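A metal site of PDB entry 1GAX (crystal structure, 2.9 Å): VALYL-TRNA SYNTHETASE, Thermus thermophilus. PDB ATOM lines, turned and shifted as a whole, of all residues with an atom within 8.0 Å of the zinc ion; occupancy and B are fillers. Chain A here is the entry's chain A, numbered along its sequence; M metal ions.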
ATOM      1  N   ILE A  85       6.233  28.120 -25.152  1.00  0.00           N
ATOM      2  CA  ILE A  85       4.984  28.169 -24.379  1.00  0.00           C
ATOM      3  C   ILE A  85       5.164  29.078 -23.159  1.00  0.00           C
ATOM      4  O   ILE A  85       4.325  29.943 -22.872  1.00  0.00           O
ATOM      5  CB  ILE A  85       4.546  26.731 -23.902  1.00  0.00           C
ATOM      6  CG1 ILE A  85       3.366  26.832 -22.931  1.00  0.00           C
ATOM      7  CG2 ILE A  85       5.687  26.017 -23.159  1.00  0.00           C
ATOM      8  CD1 ILE A  85       2.202  27.606 -23.465  1.00  0.00           C
ATOM      9  N   VAL A  89       3.221  32.690 -22.365  1.00  0.00           N
ATOM     10  CA  VAL A  89       2.380  32.979 -21.221  1.00  0.00           C
ATOM     11  C   VAL A  89       2.792  34.292 -20.577  1.00  0.00           C
ATOM     12  O   VAL A  89       2.017  35.232 -20.513  1.00  0.00           O
ATOM     13  CB  VAL A  89       2.516  31.899 -20.155  1.00  0.00           C
ATOM     14  CG1 VAL A  89       1.420  32.062 -19.123  1.00  0.00           C
ATOM     15  CG2 VAL A  89       2.480  30.529 -20.797  1.00  0.00           C
ATOM     16  N   GLU A  92       1.863  37.286 -22.623  1.00  0.00           N
ATOM     17  CA  GLU A  92       0.412  37.221 -22.796  1.00  0.00           C
ATOM     18  C   GLU A  92      -0.211  37.665 -21.478  1.00  0.00           C
ATOM     19  O   GLU A  92      -1.064  38.549 -21.436  1.00  0.00           O
ATOM     20  CB  GLU A  92       0.010  35.777 -23.117  1.00  0.00           C
ATOM     21  CG  GLU A  92      -1.346  35.570 -23.760  1.00  0.00           C
ATOM     22  CD  GLU A  92      -1.528  34.133 -24.221  1.00  0.00           C
ATOM     23  OE1 GLU A  92      -1.693  33.239 -23.358  1.00  0.00           O
ATOM     24  OE2 GLU A  92      -1.493  33.901 -25.444  1.00  0.00           O
ATOM     25  N   TRP A 175      -4.511  18.652 -25.329  1.00  0.00           N
ATOM     26  CA  TRP A 175      -4.761  20.028 -25.730  1.00  0.00           C
ATOM     27  C   TRP A 175      -5.302  20.976 -24.668  1.00  0.00           C
ATOM     28  O   TRP A 175      -6.281  20.675 -23.991  1.00  0.00           O
ATOM     29  CB  TRP A 175      -5.696  20.018 -26.954  1.00  0.00           C
ATOM     30  CG  TRP A 175      -6.437  21.305 -27.230  1.00  0.00           C
ATOM     31  CD1 TRP A 175      -7.529  21.798 -26.561  1.00  0.00           C
ATOM     32  CD2 TRP A 175      -6.110  22.277 -28.227  1.00  0.00           C
ATOM     33  NE1 TRP A 175      -7.903  23.017 -27.077  1.00  0.00           N
ATOM     34  CE2 TRP A 175      -7.050  23.338 -28.098  1.00  0.00           C
ATOM     35  CE3 TRP A 175      -5.126  22.365 -29.210  1.00  0.00           C
ATOM     36  CZ2 TRP A 175      -7.015  24.472 -28.918  1.00  0.00           C
ATOM     37  CZ3 TRP A 175      -5.086  23.491 -30.029  1.00  0.00           C
ATOM     38  CH2 TRP A 175      -6.032  24.527 -29.876  1.00  0.00           C
ATOM     39  N   CYS A 176      -4.675  22.140 -24.540  1.00  0.00           N
ATOM     40  CA  CYS A 176      -5.119  23.145 -23.590  1.00  0.00           C
ATOM     41  C   CYS A 176      -5.906  24.213 -24.327  1.00  0.00           C
ATOM     42  O   CYS A 176      -5.361  24.916 -25.180  1.00  0.00           O
ATOM     43  CB  CYS A 176      -3.941  23.821 -22.880  1.00  0.00           C
ATOM     44  SG  CYS A 176      -4.398  25.392 -22.041  1.00  0.00           S
ATOM     45  N   PRO A 177      -7.188  24.347 -24.000  1.00  0.00           N
ATOM     46  CA  PRO A 177      -8.057  25.343 -24.645  1.00  0.00           C
ATOM     47  C   PRO A 177      -7.831  26.762 -24.125  1.00  0.00           C
ATOM     48  O   PRO A 177      -8.567  27.679 -24.500  1.00  0.00           O
ATOM     49  CB  PRO A 177      -9.443  24.825 -24.332  1.00  0.00           C
ATOM     50  CG  PRO A 177      -9.252  24.232 -22.967  1.00  0.00           C
ATOM     51  CD  PRO A 177      -7.967  23.461 -23.131  1.00  0.00           C
ATOM     52  N   ARG A 178      -6.830  26.940 -23.270  1.00  0.00           N
ATOM     53  CA  ARG A 178      -6.506  28.265 -22.739  1.00  0.00           C
ATOM     54  C   ARG A 178      -5.452  28.899 -23.647  1.00  0.00           C
ATOM     55  O   ARG A 178      -5.648  29.984 -24.207  1.00  0.00           O
ATOM     56  CB  ARG A 178      -5.933  28.149 -21.308  1.00  0.00           C
ATOM     57  CG  ARG A 178      -4.567  28.835 -21.062  1.00  0.00           C
ATOM     58  CD  ARG A 178      -4.598  30.368 -21.107  1.00  0.00           C
ATOM     59  NE  ARG A 178      -5.135  30.977 -19.894  1.00  0.00           N
ATOM     60  CZ  ARG A 178      -6.396  30.890 -19.477  1.00  0.00           C
ATOM     61  NH1 ARG A 178      -7.291  30.188 -20.168  1.00  0.00           N
ATOM     62  NH2 ARG A 178      -6.777  31.496 -18.355  1.00  0.00           N
ATOM     63  N   CYS A 179      -4.355  28.186 -23.795  1.00  0.00           N
ATOM     64  CA  CYS A 179      -3.235  28.623 -24.612  1.00  0.00           C
ATOM     65  C   CYS A 179      -3.456  28.244 -26.067  1.00  0.00           C
ATOM     66  O   CYS A 179      -2.686  28.623 -26.943  1.00  0.00           O
ATOM     67  CB  CYS A 179      -1.949  27.997 -24.064  1.00  0.00           C
ATOM     68  SG  CYS A 179      -1.708  28.308 -22.296  1.00  0.00           S
ATOM     69  N   GLU A 180      -4.524  27.492 -26.321  1.00  0.00           N
ATOM     70  CA  GLU A 180      -4.849  27.064 -27.674  1.00  0.00           C
ATOM     71  C   GLU A 180      -3.599  26.445 -28.294  1.00  0.00           C
ATOM     72  O   GLU A 180      -2.964  27.035 -29.173  1.00  0.00           O
ATOM     73  CB  GLU A 180      -5.311  28.269 -28.493  1.00  0.00           C
ATOM     74  CG  GLU A 180      -6.571  28.924 -27.938  1.00  0.00           C
ATOM     75  CD  GLU A 180      -6.760  30.363 -28.387  1.00  0.00           C
ATOM     76  OE1 GLU A 180      -6.625  30.644 -29.586  1.00  0.00           O
ATOM     77  OE2 GLU A 180      -7.069  31.207 -27.533  1.00  0.00           O
ATOM     78  N   THR A 181      -3.223  25.270 -27.825  1.00  0.00           N
ATOM     79  CA  THR A 181      -2.039  24.600 -28.337  1.00  0.00           C
ATOM     80  C   THR A 181      -1.887  23.219 -27.749  1.00  0.00           C
ATOM     81  O   THR A 181      -2.390  22.933 -26.676  1.00  0.00           O
ATOM     82  CB  THR A 181      -0.788  25.335 -27.961  1.00  0.00           C
ATOM     83  OG1 THR A 181       0.330  24.450 -28.117  1.00  0.00           O
ATOM     84  CG2 THR A 181      -0.864  25.780 -26.498  1.00  0.00           C
ATOM     85  N   LEU A 183       0.282  20.149 -26.022  1.00  0.00           N
ATOM     86  CA  LEU A 183       1.380  20.033 -25.066  1.00  0.00           C
ATOM     87  C   LEU A 183       1.940  18.628 -25.188  1.00  0.00           C
ATOM     88  O   LEU A 183       1.412  17.814 -25.950  1.00  0.00           O
ATOM     89  CB  LEU A 183       0.900  20.210 -23.625  1.00  0.00           C
ATOM     90  CG  LEU A 183       0.417  21.563 -23.087  1.00  0.00           C
ATOM     91  CD1 LEU A 183      -0.773  22.062 -23.894  1.00  0.00           C
ATOM     92  CD2 LEU A 183       0.030  21.404 -21.620  1.00  0.00           C
ATOM     93  N   GLU A 187       4.876  17.942 -20.431  1.00  0.00           N
ATOM     94  CA  GLU A 187       4.431  19.305 -20.185  1.00  0.00           C
ATOM     95  C   GLU A 187       3.090  19.411 -19.490  1.00  0.00           C
ATOM     96  O   GLU A 187       2.643  20.505 -19.164  1.00  0.00           O
ATOM     97  CB  GLU A 187       4.379  20.092 -21.494  1.00  0.00           C
ATOM     98  CG  GLU A 187       5.729  20.291 -22.142  1.00  0.00           C
ATOM     99  CD  GLU A 187       5.695  21.246 -23.315  1.00  0.00           C
ATOM    100  OE1 GLU A 187       5.378  22.436 -23.121  1.00  0.00           O
ATOM    101  OE2 GLU A 187       5.992  20.799 -24.439  1.00  0.00           O
ATOM    102  N   THR A 343      -3.878  18.627 -15.975  1.00  0.00           N
ATOM    103  CA  THR A 343      -3.910  20.065 -16.220  1.00  0.00           C
ATOM    104  C   THR A 343      -2.713  20.595 -16.979  1.00  0.00           C
ATOM    105  O   THR A 343      -1.677  19.932 -17.075  1.00  0.00           O
ATOM    106  CB  THR A 343      -4.031  20.841 -14.902  1.00  0.00           C
ATOM    107  OG1 THR A 343      -2.953  20.467 -14.037  1.00  0.00           O
ATOM    108  CG2 THR A 343      -5.351  20.513 -14.218  1.00  0.00           C
ATOM    109  N   CYS A 344      -2.859  21.811 -17.513  1.00  0.00           N
ATOM    110  CA  CYS A 344      -1.775  22.451 -18.263  1.00  0.00           C
ATOM    111  C   CYS A 344      -0.735  22.990 -17.291  1.00  0.00           C
ATOM    112  O   CYS A 344      -0.993  23.965 -16.575  1.00  0.00           O
ATOM    113  CB  CYS A 344      -2.317  23.598 -19.113  1.00  0.00           C
ATOM    114  SG  CYS A 344      -1.068  24.268 -20.214  1.00  0.00           S
ATOM    115  N   SER A 345       0.438  22.364 -17.289  1.00  0.00           N
ATOM    116  CA  SER A 345       1.501  22.752 -16.370  1.00  0.00           C
ATOM    117  C   SER A 345       1.798  24.252 -16.360  1.00  0.00           C
ATOM    118  O   SER A 345       2.152  24.810 -15.315  1.00  0.00           O
ATOM    119  CB  SER A 345       2.794  21.997 -16.680  1.00  0.00           C
ATOM    120  OG  SER A 345       3.536  22.634 -17.702  1.00  0.00           O
ATOM    121  N   ARG A 346       1.649  24.919 -17.497  1.00  0.00           N
ATOM    122  CA  ARG A 346       1.959  26.330 -17.547  1.00  0.00           C
ATOM    123  C   ARG A 346       0.809  27.336 -17.516  1.00  0.00           C
ATOM    124  O   ARG A 346       1.035  28.533 -17.687  1.00  0.00           O
ATOM    125  CB  ARG A 346       2.881  26.608 -18.733  1.00  0.00           C
ATOM    126  CG  ARG A 346       3.810  27.785 -18.502  1.00  0.00           C
ATOM    127  CD  ARG A 346       5.223  27.549 -19.014  1.00  0.00           C
ATOM    128  NE  ARG A 346       5.932  26.443 -18.364  1.00  0.00           N
ATOM    129  CZ  ARG A 346       5.882  25.176 -18.755  1.00  0.00           C
ATOM    130  NH1 ARG A 346       5.154  24.824 -19.803  1.00  0.00           N
ATOM    131  NH2 ARG A 346       6.587  24.250 -18.109  1.00  0.00           N
ATOM    132  N   CYS A 347      -0.421  26.874 -17.303  1.00  0.00           N
ATOM    133  CA  CYS A 347      -1.555  27.801 -17.232  1.00  0.00           C
ATOM    134  C   CYS A 347      -2.603  27.336 -16.247  1.00  0.00           C
ATOM    135  O   CYS A 347      -3.534  28.085 -15.921  1.00  0.00           O
ATOM    136  CB  CYS A 347      -2.220  27.985 -18.599  1.00  0.00           C
ATOM    137  SG  CYS A 347      -3.753  27.048 -18.850  1.00  0.00           S
ATOM    138  N   GLY A 348      -2.470  26.096 -15.779  1.00  0.00           N
ATOM    139  CA  GLY A 348      -3.425  25.577 -14.819  1.00  0.00           C
ATOM    140  C   GLY A 348      -4.589  24.793 -15.403  1.00  0.00           C
ATOM    141  O   GLY A 348      -4.713  23.591 -15.141  1.00  0.00           O
ATOM    142  N   THR A 349      -5.449  25.464 -16.174  1.00  0.00           N
ATOM    143  CA  THR A 349      -6.608  24.829 -16.801  1.00  0.00           C
ATOM    144  C   THR A 349      -6.370  23.347 -17.126  1.00  0.00           C
ATOM    145  O   THR A 349      -5.287  22.957 -17.574  1.00  0.00           O
ATOM    146  CB  THR A 349      -6.995  25.545 -18.128  1.00  0.00           C
ATOM    147  OG1 THR A 349      -7.255  26.930 -17.878  1.00  0.00           O
ATOM    148  CG2 THR A 349      -8.221  24.908 -18.746  1.00  0.00           C
ATOM    149  N   PRO A 350      -7.388  22.499 -16.884  1.00  0.00           N
ATOM    150  CA  PRO A 350      -7.240  21.074 -17.165  1.00  0.00           C
ATOM    151  C   PRO A 350      -7.234  20.872 -18.674  1.00  0.00           C
ATOM    152  O   PRO A 350      -7.992  21.523 -19.395  1.00  0.00           O
ATOM    153  CB  PRO A 350      -8.463  20.466 -16.504  1.00  0.00           C
ATOM    154  CG  PRO A 350      -9.497  21.529 -16.720  1.00  0.00           C
ATOM    155  CD  PRO A 350      -8.732  22.795 -16.379  1.00  0.00           C
ATOM    156  N   ILE A 351      -6.365  19.987 -19.146  1.00  0.00           N
ATOM    157  CA  ILE A 351      -6.227  19.705 -20.558  1.00  0.00           C
ATOM    158  C   ILE A 351      -7.523  19.265 -21.236  1.00  0.00           C
ATOM    159  O   ILE A 351      -8.610  19.787 -20.970  1.00  0.00           O
ATOM    160  CB  ILE A 351      -5.161  18.625 -20.802  1.00  0.00           C
ATOM    161  CG1 ILE A 351      -5.539  17.356 -20.041  1.00  0.00           C
ATOM    162  CG2 ILE A 351      -3.803  19.115 -20.373  1.00  0.00           C
ATOM    163  CD1 ILE A 351      -4.688  16.161 -20.394  1.00  0.00           C
HETATM  164 ZN    ZN M   1      -2.361  26.286 -20.729  1.00  0.00          ZN
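The backbone NH of Cys 176 is in hydrogen-bond range of the backbone carbonyl oxygen of Thr 181 (3.2 Å).
N of Arg 178 lies close to SG of Cys 176, at 3.1 Å.
The backbone NH (N) of Thr 349 lies close to the side-chain sulfur (SG) of Cys 347 (3.5 Å).
The backbone NH of Cys 344 is in hydrogen-bond range of the backbone carbonyl oxygen of Thr 349.
Residues that only touch the zinc ion: Arg 178 (3.4 Å).
Of the 21 residues printed, 5 come within 4 Å of the zinc ion.
The side-chain sulfur (SG) of Cys 344 is bound to the zinc ion (2.5 Å).
The zinc ion is bound by SG of Cys 347, 2.5 Å away.
SG of Cys 176 is bound to the zinc ion, at 2.6 Å.
The zinc ion is bound by SG of Cys 179, at 2.6 Å.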
